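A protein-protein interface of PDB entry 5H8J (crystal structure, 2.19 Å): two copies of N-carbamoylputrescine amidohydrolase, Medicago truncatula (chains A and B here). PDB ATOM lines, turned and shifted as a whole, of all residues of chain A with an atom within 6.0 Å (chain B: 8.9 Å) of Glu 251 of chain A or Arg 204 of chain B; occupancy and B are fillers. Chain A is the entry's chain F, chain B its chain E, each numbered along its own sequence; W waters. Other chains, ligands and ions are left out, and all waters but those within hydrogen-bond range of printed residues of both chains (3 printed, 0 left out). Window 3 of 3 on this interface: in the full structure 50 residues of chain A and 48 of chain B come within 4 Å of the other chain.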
ATOM      1  N   ARG A 204       1.254  -9.725  13.057  1.00  0.00           N
ATOM      2  CA  ARG A 204       1.969  -8.533  12.628  1.00  0.00           C
ATOM      3  C   ARG A 204       1.036  -7.351  12.390  1.00  0.00           C
ATOM      4  O   ARG A 204       1.326  -6.250  12.796  1.00  0.00           O
ATOM      5  CB  ARG A 204       2.841  -8.808  11.407  1.00  0.00           C
ATOM      6  CG  ARG A 204       4.056  -9.630  11.732  1.00  0.00           C
ATOM      7  CD  ARG A 204       5.041  -9.692  10.570  1.00  0.00           C
ATOM      8  NE  ARG A 204       4.513 -10.455   9.428  1.00  0.00           N
ATOM      9  CZ  ARG A 204       4.872 -11.707   9.118  1.00  0.00           C
ATOM     10  NH1 ARG A 204       5.778 -12.348   9.854  1.00  0.00           N
ATOM     11  NH2 ARG A 204       4.330 -12.311   8.067  1.00  0.00           N
ATOM     12  N   GLN A 207      -0.026  -6.162  15.840  1.00  0.00           N
ATOM     13  CA  GLN A 207       1.082  -5.561  16.541  1.00  0.00           C
ATOM     14  C   GLN A 207       1.278  -4.152  15.987  1.00  0.00           C
ATOM     15  O   GLN A 207       1.640  -3.212  16.719  1.00  0.00           O
ATOM     16  CB  GLN A 207       2.321  -6.363  16.360  1.00  0.00           C
ATOM     17  CG  GLN A 207       2.310  -7.667  17.116  1.00  0.00           C
ATOM     18  CD  GLN A 207       3.489  -8.533  16.750  1.00  0.00           C
ATOM     19  OE1 GLN A 207       3.426  -9.289  15.787  1.00  0.00           O
ATOM     20  NE2 GLN A 207       4.564  -8.436  17.519  1.00  0.00           N
ATOM     21  N   GLY A 208       1.037  -4.006  14.681  1.00  0.00           N
ATOM     22  CA  GLY A 208       1.110  -2.714  14.040  1.00  0.00           C
ATOM     23  C   GLY A 208       0.149  -1.700  14.670  1.00  0.00           C
ATOM     24  O   GLY A 208       0.536  -0.560  14.928  1.00  0.00           O
ATOM     25  N   ILE A 245      -1.460 -11.122  23.857  1.00  0.00           N
ATOM     26  CA  ILE A 245      -1.526  -9.792  24.460  1.00  0.00           C
ATOM     27  C   ILE A 245      -0.261  -9.052  24.048  1.00  0.00           C
ATOM     28  O   ILE A 245       0.827  -9.531  24.243  1.00  0.00           O
ATOM     29  CB  ILE A 245      -1.563  -9.829  25.995  1.00  0.00           C
ATOM     30  CG1 ILE A 245      -2.754 -10.649  26.484  1.00  0.00           C
ATOM     31  CG2 ILE A 245      -1.635  -8.377  26.557  1.00  0.00           C
ATOM     32  CD1 ILE A 245      -2.729 -10.857  27.994  1.00  0.00           C
ATOM     33  N   ALA A 246      -0.449  -7.880  23.464  1.00  0.00           N
ATOM     34  CA  ALA A 246       0.643  -7.015  23.026  1.00  0.00           C
ATOM     35  C   ALA A 246       0.645  -5.696  23.803  1.00  0.00           C
ATOM     36  O   ALA A 246      -0.421  -5.170  24.138  1.00  0.00           O
ATOM     37  CB  ALA A 246       0.506  -6.716  21.551  1.00  0.00           C
ATOM     38  N   GLY A 247       1.850  -5.186  24.063  1.00  0.00           N
ATOM     39  CA  GLY A 247       2.050  -3.926  24.720  1.00  0.00           C
ATOM     40  C   GLY A 247       1.977  -2.752  23.762  1.00  0.00           C
ATOM     41  O   GLY A 247       1.843  -2.924  22.534  1.00  0.00           O
ATOM     42  N   PRO A 248       2.076  -1.535  24.301  1.00  0.00           N
ATOM     43  CA  PRO A 248       1.914  -0.339  23.489  1.00  0.00           C
ATOM     44  C   PRO A 248       3.041  -0.054  22.447  1.00  0.00           C
ATOM     45  O   PRO A 248       2.931   0.908  21.726  1.00  0.00           O
ATOM     46  CB  PRO A 248       1.805   0.767  24.529  1.00  0.00           C
ATOM     47  CG  PRO A 248       2.632   0.279  25.694  1.00  0.00           C
ATOM     48  CD  PRO A 248       2.382  -1.212  25.711  1.00  0.00           C
ATOM     49  N   THR A 249       4.089  -0.861  22.381  1.00  0.00           N
ATOM     50  CA  THR A 249       5.031  -0.739  21.264  1.00  0.00           C
ATOM     51  C   THR A 249       4.853  -1.941  20.269  1.00  0.00           C
ATOM     52  O   THR A 249       5.632  -2.113  19.303  1.00  0.00           O
ATOM     53  CB  THR A 249       6.497  -0.690  21.709  1.00  0.00           C
ATOM     54  OG1 THR A 249       6.837  -1.905  22.360  1.00  0.00           O
ATOM     55  CG2 THR A 249       6.767   0.543  22.657  1.00  0.00           C
ATOM     56  N   GLY A 250       3.845  -2.762  20.509  1.00  0.00           N
ATOM     57  CA  GLY A 250       3.594  -3.915  19.642  1.00  0.00           C
ATOM     58  C   GLY A 250       4.278  -5.177  20.090  1.00  0.00           C
ATOM     59  O   GLY A 250       4.068  -6.213  19.485  1.00  0.00           O
ATOM     60  N   GLU A 251       5.095  -5.095  21.146  1.00  0.00           N
ATOM     61  CA  GLU A 251       5.782  -6.282  21.673  1.00  0.00           C
ATOM     62  C   GLU A 251       4.770  -7.298  22.248  1.00  0.00           C
ATOM     63  O   GLU A 251       3.866  -6.924  23.001  1.00  0.00           O
ATOM     64  CB  GLU A 251       6.824  -5.902  22.741  1.00  0.00           C
ATOM     65  CG  GLU A 251       7.519  -7.135  23.291  1.00  0.00           C
ATOM     66  CD  GLU A 251       8.806  -6.891  24.061  1.00  0.00           C
ATOM     67  OE1 GLU A 251       9.428  -5.832  23.867  1.00  0.00           O
ATOM     68  OE2 GLU A 251       9.205  -7.770  24.850  1.00  0.00           O
ATOM     69  N   ILE A 252       4.915  -8.572  21.873  1.00  0.00           N
ATOM     70  CA  ILE A 252       4.042  -9.626  22.422  1.00  0.00           C
ATOM     71  C   ILE A 252       4.531  -9.895  23.831  1.00  0.00           C
ATOM     72  O   ILE A 252       5.677 -10.306  23.997  1.00  0.00           O
ATOM     73  CB  ILE A 252       4.176 -10.979  21.666  1.00  0.00           C
ATOM     74  CG1 ILE A 252       3.754 -10.876  20.196  1.00  0.00           C
ATOM     75  CG2 ILE A 252       3.380 -12.072  22.370  1.00  0.00           C
ATOM     76  CD1 ILE A 252       2.303 -10.645  19.955  1.00  0.00           C
ATOM     77  N   VAL A 253       3.684  -9.678  24.834  1.00  0.00           N
ATOM     78  CA  VAL A 253       4.051  -9.969  26.233  1.00  0.00           C
ATOM     79  C   VAL A 253       3.564 -11.334  26.734  1.00  0.00           C
ATOM     80  O   VAL A 253       4.153 -11.928  27.624  1.00  0.00           O
ATOM     81  CB  VAL A 253       3.618  -8.849  27.207  1.00  0.00           C
ATOM     82  CG1 VAL A 253       4.442  -7.591  26.935  1.00  0.00           C
ATOM     83  CG2 VAL A 253       2.133  -8.529  27.091  1.00  0.00           C
ATOM     84  N   SER A 254       2.496 -11.823  26.140  1.00  0.00           N
ATOM     85  CA  SER A 254       1.912 -13.093  26.522  1.00  0.00           C
ATOM     86  C   SER A 254       1.383 -13.699  25.253  1.00  0.00           C
ATOM     87  O   SER A 254       0.801 -12.978  24.423  1.00  0.00           O
ATOM     88  CB  SER A 254       0.762 -12.835  27.510  1.00  0.00           C
ATOM     89  OG  SER A 254       0.307 -14.033  28.106  1.00  0.00           O
ATOM     90  N   GLN B 164       6.332   7.309   8.253  1.00  0.00           N
ATOM     91  CA  GLN B 164       6.286   5.838   8.399  1.00  0.00           C
ATOM     92  C   GLN B 164       5.544   5.341   9.623  1.00  0.00           C
ATOM     93  O   GLN B 164       5.220   4.190   9.706  1.00  0.00           O
ATOM     94  CB  GLN B 164       7.716   5.218   8.338  1.00  0.00           C
ATOM     95  CG  GLN B 164       8.535   5.412   9.587  1.00  0.00           C
ATOM     96  CD  GLN B 164      10.046   5.502   9.372  1.00  0.00           C
ATOM     97  OE1 GLN B 164      10.721   6.109  10.153  1.00  0.00           O
ATOM     98  NE2 GLN B 164      10.566   4.882   8.309  1.00  0.00           N
ATOM     99  N   TRP B 165       5.270   6.197  10.567  1.00  0.00           N
ATOM    100  CA  TRP B 165       4.571   5.772  11.782  1.00  0.00           C
ATOM    101  C   TRP B 165       3.042   5.837  11.643  1.00  0.00           C
ATOM    102  O   TRP B 165       2.297   5.326  12.524  1.00  0.00           O
ATOM    103  CB  TRP B 165       5.023   6.642  12.952  1.00  0.00           C
ATOM    104  CG  TRP B 165       6.480   6.413  13.363  1.00  0.00           C
ATOM    105  CD1 TRP B 165       7.599   7.029  12.844  1.00  0.00           C
ATOM    106  CD2 TRP B 165       6.972   5.517  14.382  1.00  0.00           C
ATOM    107  NE1 TRP B 165       8.761   6.557  13.484  1.00  0.00           N
ATOM    108  CE2 TRP B 165       8.396   5.635  14.419  1.00  0.00           C
ATOM    109  CE3 TRP B 165       6.362   4.628  15.250  1.00  0.00           C
ATOM    110  CZ2 TRP B 165       9.181   4.893  15.291  1.00  0.00           C
ATOM    111  CZ3 TRP B 165       7.148   3.905  16.108  1.00  0.00           C
ATOM    112  CH2 TRP B 165       8.547   4.046  16.132  1.00  0.00           C
ATOM    113  N   PRO B 167      -0.427   4.881   9.827  1.00  0.00           N
ATOM    114  CA  PRO B 167      -1.178   3.965   8.958  1.00  0.00           C
ATOM    115  C   PRO B 167      -1.959   4.729   7.920  1.00  0.00           C
ATOM    116  O   PRO B 167      -2.186   4.222   6.865  1.00  0.00           O
ATOM    117  CB  PRO B 167      -2.108   3.242   9.931  1.00  0.00           C
ATOM    118  CG  PRO B 167      -1.338   3.274  11.221  1.00  0.00           C
ATOM    119  CD  PRO B 167      -0.754   4.645  11.254  1.00  0.00           C
ATOM    120  N   ASP B 197      15.116   3.210  23.095  1.00  0.00           N
ATOM    121  CA  ASP B 197      15.594   2.384  21.973  1.00  0.00           C
ATOM    122  C   ASP B 197      14.352   2.014  21.155  1.00  0.00           C
ATOM    123  O   ASP B 197      13.625   1.110  21.482  1.00  0.00           O
ATOM    124  CB  ASP B 197      16.345   1.154  22.487  1.00  0.00           C
ATOM    125  CG  ASP B 197      16.758   0.206  21.356  1.00  0.00           C
ATOM    126  OD1 ASP B 197      16.410   0.489  20.160  1.00  0.00           O
ATOM    127  OD2 ASP B 197      17.416  -0.812  21.652  1.00  0.00           O
ATOM    128  N   SER B 198      14.139   2.737  20.080  1.00  0.00           N
ATOM    129  CA  SER B 198      12.912   2.636  19.346  1.00  0.00           C
ATOM    130  C   SER B 198      12.924   1.680  18.175  1.00  0.00           C
ATOM    131  O   SER B 198      11.919   1.559  17.536  1.00  0.00           O
ATOM    132  CB  SER B 198      12.531   4.044  18.837  1.00  0.00           C
ATOM    133  OG  SER B 198      13.506   4.518  17.906  1.00  0.00           O
ATOM    134  N   ARG B 199      14.057   1.007  17.910  1.00  0.00           N
ATOM    135  CA  ARG B 199      14.224   0.208  16.666  1.00  0.00           C
ATOM    136  C   ARG B 199      13.194  -0.897  16.462  1.00  0.00           C
ATOM    137  O   ARG B 199      12.734  -1.103  15.320  1.00  0.00           O
ATOM    138  CB  ARG B 199      15.654  -0.327  16.517  1.00  0.00           C
ATOM    139  CG  ARG B 199      16.004  -1.563  17.376  1.00  0.00           C
ATOM    140  CD  ARG B 199      17.508  -1.780  17.439  1.00  0.00           C
ATOM    141  NE  ARG B 199      18.128  -0.681  18.200  1.00  0.00           N
ATOM    142  CZ  ARG B 199      19.441  -0.395  18.194  1.00  0.00           C
ATOM    143  NH1 ARG B 199      20.288  -1.125  17.460  1.00  0.00           N
ATOM    144  NH2 ARG B 199      19.898   0.615  18.906  1.00  0.00           N
ATOM    145  N   ASP B 200      12.827  -1.592  17.537  1.00  0.00           N
ATOM    146  CA  ASP B 200      11.877  -2.680  17.457  1.00  0.00           C
ATOM    147  C   ASP B 200      10.459  -2.204  17.174  1.00  0.00           C
ATOM    148  O   ASP B 200       9.750  -2.781  16.339  1.00  0.00           O
ATOM    149  CB  ASP B 200      11.925  -3.533  18.714  1.00  0.00           C
ATOM    150  CG  ASP B 200      13.137  -4.470  18.729  1.00  0.00           C
ATOM    151  OD1 ASP B 200      13.598  -4.871  17.623  1.00  0.00           O
ATOM    152  OD2 ASP B 200      13.617  -4.815  19.837  1.00  0.00           O
ATOM    153  N   HIS B 201      10.072  -1.169  17.881  1.00  0.00           N
ATOM    154  CA  HIS B 201       8.796  -0.483  17.723  1.00  0.00           C
ATOM    155  C   HIS B 201       8.635   0.052  16.307  1.00  0.00           C
ATOM    156  O   HIS B 201       7.567  -0.116  15.684  1.00  0.00           O
ATOM    157  CB  HIS B 201       8.776   0.677  18.721  1.00  0.00           C
ATOM    158  CG  HIS B 201       7.500   1.421  18.789  1.00  0.00           C
ATOM    159  ND1 HIS B 201       7.395   2.636  19.416  1.00  0.00           N
ATOM    160  CD2 HIS B 201       6.266   1.130  18.321  1.00  0.00           C
ATOM    161  CE1 HIS B 201       6.154   3.061  19.343  1.00  0.00           C
ATOM    162  NE2 HIS B 201       5.446   2.164  18.675  1.00  0.00           N
ATOM    163  N   TRP B 202       9.706   0.702  15.823  1.00  0.00           N
ATOM    164  CA  TRP B 202       9.803   1.302  14.489  1.00  0.00           C
ATOM    165  C   TRP B 202       9.523   0.260  13.375  1.00  0.00           C
ATOM    166  O   TRP B 202       8.734   0.542  12.448  1.00  0.00           O
ATOM    167  CB  TRP B 202      11.200   1.941  14.353  1.00  0.00           C
ATOM    168  CG  TRP B 202      11.640   2.495  13.046  1.00  0.00           C
ATOM    169  CD1 TRP B 202      11.233   3.693  12.437  1.00  0.00           C
ATOM    170  CD2 TRP B 202      12.613   1.922  12.169  1.00  0.00           C
ATOM    171  NE1 TRP B 202      11.895   3.854  11.254  1.00  0.00           N
ATOM    172  CE2 TRP B 202      12.741   2.786  11.060  1.00  0.00           C
ATOM    173  CE3 TRP B 202      13.379   0.765  12.206  1.00  0.00           C
ATOM    174  CZ2 TRP B 202      13.613   2.502   9.987  1.00  0.00           C
ATOM    175  CZ3 TRP B 202      14.255   0.493  11.154  1.00  0.00           C
ATOM    176  CH2 TRP B 202      14.364   1.348  10.067  1.00  0.00           C
ATOM    177  N   LYS B 203      10.153  -0.914  13.487  1.00  0.00           N
ATOM    178  CA  LYS B 203       9.970  -1.997  12.524  1.00  0.00           C
ATOM    179  C   LYS B 203       8.545  -2.543  12.537  1.00  0.00           C
ATOM    180  O   LYS B 203       7.897  -2.659  11.496  1.00  0.00           O
ATOM    181  CB  LYS B 203      10.981  -3.137  12.759  1.00  0.00           C
ATOM    182  CG  LYS B 203      12.337  -2.815  12.208  1.00  0.00           C
ATOM    183  CD  LYS B 203      13.356  -3.923  12.380  1.00  0.00           C
ATOM    184  CE  LYS B 203      13.896  -3.928  13.775  1.00  0.00           C
ATOM    185  NZ  LYS B 203      15.079  -4.817  13.904  1.00  0.00           N
ATOM    186  N   ARG B 204       8.061  -2.851  13.728  1.00  0.00           N
ATOM    187  CA  ARG B 204       6.705  -3.422  13.899  1.00  0.00           C
ATOM    188  C   ARG B 204       5.587  -2.541  13.296  1.00  0.00           C
ATOM    189  O   ARG B 204       4.681  -3.034  12.648  1.00  0.00           O
ATOM    190  CB  ARG B 204       6.414  -3.710  15.386  1.00  0.00           C
ATOM    191  CG  ARG B 204       7.179  -4.904  15.949  1.00  0.00           C
ATOM    192  CD  ARG B 204       6.667  -5.385  17.313  1.00  0.00           C
ATOM    193  NE  ARG B 204       7.042  -4.416  18.340  1.00  0.00           N
ATOM    194  CZ  ARG B 204       8.050  -4.575  19.200  1.00  0.00           C
ATOM    195  NH1 ARG B 204       8.768  -5.684  19.189  1.00  0.00           N
ATOM    196  NH2 ARG B 204       8.314  -3.644  20.065  1.00  0.00           N
ATOM    197  N   VAL B 205       5.664  -1.237  13.502  1.00  0.00           N
ATOM    198  CA  VAL B 205       4.653  -0.360  12.983  1.00  0.00           C
ATOM    199  C   VAL B 205       4.645  -0.422  11.434  1.00  0.00           C
ATOM    200  O   VAL B 205       3.588  -0.474  10.805  1.00  0.00           O
ATOM    201  CB  VAL B 205       4.874   1.055  13.492  1.00  0.00           C
ATOM    202  CG1 VAL B 205       3.996   2.060  12.747  1.00  0.00           C
ATOM    203  CG2 VAL B 205       4.601   1.112  14.994  1.00  0.00           C
ATOM    204  N   MET B 206       5.846  -0.415  10.841  1.00  0.00           N
ATOM    205  CA  MET B 206       5.967  -0.515   9.388  1.00  0.00           C
ATOM    206  C   MET B 206       5.536  -1.866   8.844  1.00  0.00           C
ATOM    207  O   MET B 206       4.905  -1.912   7.818  1.00  0.00           O
ATOM    208  CB  MET B 206       7.358  -0.120   8.881  1.00  0.00           C
ATOM    209  CG  MET B 206       7.489   1.362   8.654  1.00  0.00           C
ATOM    210  SD  MET B 206       9.105   1.835   8.009  1.00  0.00           S
ATOM    211  CE  MET B 206      10.155   1.481   9.417  1.00  0.00           C
ATOM    212  N   GLN B 207       5.868  -2.940   9.543  1.00  0.00           N
ATOM    213  CA  GLN B 207       5.447  -4.270   9.132  1.00  0.00           C
ATOM    214  C   GLN B 207       3.936  -4.316   9.129  1.00  0.00           C
ATOM    215  O   GLN B 207       3.324  -5.002   8.334  1.00  0.00           O
ATOM    216  CB  GLN B 207       5.991  -5.339  10.082  1.00  0.00           C
ATOM    217  CG  GLN B 207       7.490  -5.596   9.947  1.00  0.00           C
ATOM    218  CD  GLN B 207       8.029  -6.578  10.992  1.00  0.00           C
ATOM    219  OE1 GLN B 207       8.395  -6.193  12.106  1.00  0.00           O
ATOM    220  NE2 GLN B 207       8.093  -7.821  10.632  1.00  0.00           N
ATOM    221  N   GLY B 208       3.333  -3.571  10.038  1.00  0.00           N
ATOM    222  CA  GLY B 208       1.897  -3.503  10.112  1.00  0.00           C
ATOM    223  C   GLY B 208       1.296  -2.876   8.853  1.00  0.00           C
ATOM    224  O   GLY B 208       0.287  -3.373   8.331  1.00  0.00           O
ATOM    225  N   HIS B 209       1.908  -1.785   8.373  1.00  0.00           N
ATOM    226  CA  HIS B 209       1.427  -1.159   7.173  1.00  0.00           C
ATOM    227  C   HIS B 209       1.541  -2.100   5.980  1.00  0.00           C
ATOM    228  O   HIS B 209       0.605  -2.167   5.137  1.00  0.00           O
ATOM    229  CB  HIS B 209       2.195   0.077   6.781  1.00  0.00           C
ATOM    230  CG  HIS B 209       2.331   1.089   7.856  1.00  0.00           C
ATOM    231  ND1 HIS B 209       1.374   1.292   8.827  1.00  0.00           N
ATOM    232  CD2 HIS B 209       3.305   1.980   8.089  1.00  0.00           C
ATOM    233  CE1 HIS B 209       1.774   2.248   9.634  1.00  0.00           C
ATOM    234  NE2 HIS B 209       2.936   2.692   9.199  1.00  0.00           N
ATOM    235  N   ALA B 210       2.678  -2.803   5.890  1.00  0.00           N
ATOM    236  CA  ALA B 210       2.880  -3.695   4.778  1.00  0.00           C
ATOM    237  C   ALA B 210       1.834  -4.850   4.822  1.00  0.00           C
ATOM    238  O   ALA B 210       1.225  -5.186   3.801  1.00  0.00           O
ATOM    239  CB  ALA B 210       4.296  -4.202   4.766  1.00  0.00           C
ATOM    240  N   GLY B 211       1.605  -5.431   5.997  1.00  0.00           N
ATOM    241  CA  GLY B 211       0.603  -6.504   6.114  1.00  0.00           C
ATOM    242  C   GLY B 211      -0.871  -6.073   5.953  1.00  0.00           C
ATOM    243  O   GLY B 211      -1.706  -6.824   5.438  1.00  0.00           O
ATOM    244  N   ALA B 212      -1.200  -4.875   6.406  1.00  0.00           N
ATOM    245  CA  ALA B 212      -2.568  -4.379   6.313  1.00  0.00           C
ATOM    246  C   ALA B 212      -2.956  -3.945   4.908  1.00  0.00           C
ATOM    247  O   ALA B 212      -4.150  -3.934   4.572  1.00  0.00           O
ATOM    248  CB  ALA B 212      -2.766  -3.201   7.279  1.00  0.00           C
ATOM    249  N   LEU B 217       7.341  -3.229   1.364  1.00  0.00           N
ATOM    250  CA  LEU B 217       7.754  -1.945   1.960  1.00  0.00           C
ATOM    251  C   LEU B 217       9.258  -1.905   2.156  1.00  0.00           C
ATOM    252  O   LEU B 217       9.882  -2.884   2.603  1.00  0.00           O
ATOM    253  CB  LEU B 217       6.984  -1.749   3.230  1.00  0.00           C
ATOM    254  CG  LEU B 217       7.236  -0.531   4.088  1.00  0.00           C
ATOM    255  CD1 LEU B 217       6.046  -0.238   4.981  1.00  0.00           C
ATOM    256  CD2 LEU B 217       8.512  -0.648   4.915  1.00  0.00           C
ATOM    257  N   PHE B 244      15.602  -2.175   6.081  1.00  0.00           N
ATOM    258  CA  PHE B 244      14.997  -3.459   5.791  1.00  0.00           C
ATOM    259  C   PHE B 244      14.018  -3.446   4.639  1.00  0.00           C
ATOM    260  O   PHE B 244      13.545  -2.410   4.224  1.00  0.00           O
ATOM    261  CB  PHE B 244      14.317  -4.031   7.059  1.00  0.00           C
ATOM    262  CG  PHE B 244      13.063  -3.311   7.455  1.00  0.00           C
ATOM    263  CD1 PHE B 244      11.827  -3.713   6.941  1.00  0.00           C
ATOM    264  CD2 PHE B 244      13.107  -2.270   8.305  1.00  0.00           C
ATOM    265  CE1 PHE B 244      10.667  -3.063   7.288  1.00  0.00           C
ATOM    266  CE2 PHE B 244      11.933  -1.582   8.677  1.00  0.00           C
ATOM    267  CZ  PHE B 244      10.704  -1.980   8.169  1.00  0.00           C
ATOM    268  N   ALA B 246      10.388  -5.435   3.650  1.00  0.00           N
ATOM    269  CA  ALA B 246       9.309  -6.318   4.122  1.00  0.00           C
ATOM    270  C   ALA B 246       8.403  -6.693   2.981  1.00  0.00           C
ATOM    271  O   ALA B 246       8.080  -5.852   2.133  1.00  0.00           O
ATOM    272  CB  ALA B 246       8.486  -5.612   5.148  1.00  0.00           C
ATOM    273  N   GLY B 250       4.055  -8.596   5.706  1.00  0.00           N
ATOM    274  CA  GLY B 250       4.839  -7.964   6.767  1.00  0.00           C
ATOM    275  C   GLY B 250       6.144  -8.646   7.181  1.00  0.00           C
ATOM    276  O   GLY B 250       6.908  -8.071   7.966  1.00  0.00           O
ATOM    277  N   ILE B 252       9.917  -9.774   7.256  1.00  0.00           N
ATOM    278  CA  ILE B 252      11.147  -9.116   6.837  1.00  0.00           C
ATOM    279  C   ILE B 252      11.887 -10.084   5.924  1.00  0.00           C
ATOM    280  O   ILE B 252      12.165 -11.170   6.322  1.00  0.00           O
ATOM    281  CB  ILE B 252      12.078  -8.802   8.063  1.00  0.00           C
ATOM    282  CG1 ILE B 252      11.353  -8.012   9.151  1.00  0.00           C
ATOM    283  CG2 ILE B 252      13.356  -8.078   7.637  1.00  0.00           C
ATOM    284  CD1 ILE B 252      10.917  -6.656   8.726  1.00  0.00           C
HETATM  285  O   HOH W   1       0.907  -0.063  12.106  1.00  0.00           O
HETATM  286  O   HOH W   2       4.024  -5.582  13.173  1.00  0.00           O
HETATM  287  O   HOH W   3      10.856  -5.570  21.319  1.00  0.00           O
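Water W2 lies within hydrogen-bond range of O of Arg 204 of chain B and O of Arg 204 of chain A. Water W1 lies within hydrogen-bond range of O of Gly 208 of chain A and O of Val 205 of chain B. Water W3 lies within hydrogen-bond range of OE1 of Glu 251 of chain A (2.9 Å), NH1 of Arg 204 of chain B (3.0 Å) and OD2 of Asp 200 of chain B (3.2 Å).
The backbone carbonyl oxygen (O) of Thr 249 of chain A lies within hydrogen-bond range of the guanidinium group (NE) of Arg 204 of chain B (2.9 Å). N of Glu 251 of chain A lies close to NE of Arg 204 of chain B (3.5 Å).
Of chain B, only Arg 204 (3.5 Å) comes within 4 Å of Glu 251 of chain A. Arg 204 of chain B touches five residues of chain A. Ala 246 of chain A touches none of the printed residues of chain B. No residue of chain B comes within 4 Å of Gly 247 of chain A. Of the printed residues of chain A, Gly 250 of chain B touches Arg 204 (3.3 Å). Printed residues of chain A within 4 Å of Gln 207 of chain B: Arg 204. Ile 252 of chain B touches none of the printed residues of chain A. Ser 198 of chain B touches none of the printed residues of chain A. The nearest printed residue of chain A that does not touch Gly 208 of chain B is Gly 208 of chain A (4.1 Å).
The backbone carbonyl oxygen of Gly 250 of chain B lies within hydrogen-bond range of the side-chain amide nitrogen of Gln 207 of chain B. NE2 of Gln 207 of chain A lies within hydrogen-bond range of O of Gly 250 of chain A.
Hydrophobic or aromatic side chains of chain B that line the printed part of chain A: His 201. Among the printed residues, 9 pairs touch across the chains. Among the printed residues, no Asp or Glu carboxylate lies within 4 Å of a Lys or Arg side-chain nitrogen of the other chain.
Arg 204 of chain A touches Gln 207 of chain B, and with the chains exchanged Gln 207 of chain A touches Arg 204 of chain B. Arg 204 of chain A touches Gly 208 of chain B, and with the chains exchanged Gly 208 of chain A touches Arg 204 of chain B. Arg 204 of chain A touches Gly 250 of chain B, and with the chains exchanged Gly 250 of chain A touches Arg 204 of chain B. Positions printed for both chains: 204, 207, 208, 246, 250 and 252.
Gln 207 of chain B touches Arg 204 of chain A (NE2 to CD, 3.6 Å). Gly 208 of chain B touches Arg 204 of chain A. Gly 250 of chain B touches Arg 204 of chain A (C to NE, 3.3 Å). Gln 207 of chain A touches Arg 204 of chain B (NE2 to CD, 3.7 Å). CA of Gly 208 of chain A touches O of Arg 204 of chain B (3.8 Å). O of Thr 249 of chain A touches CD2 of His 201 of chain B (3.4 Å). C of Gly 250 of chain A touches NE of Arg 204 of chain B (3.4 Å).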
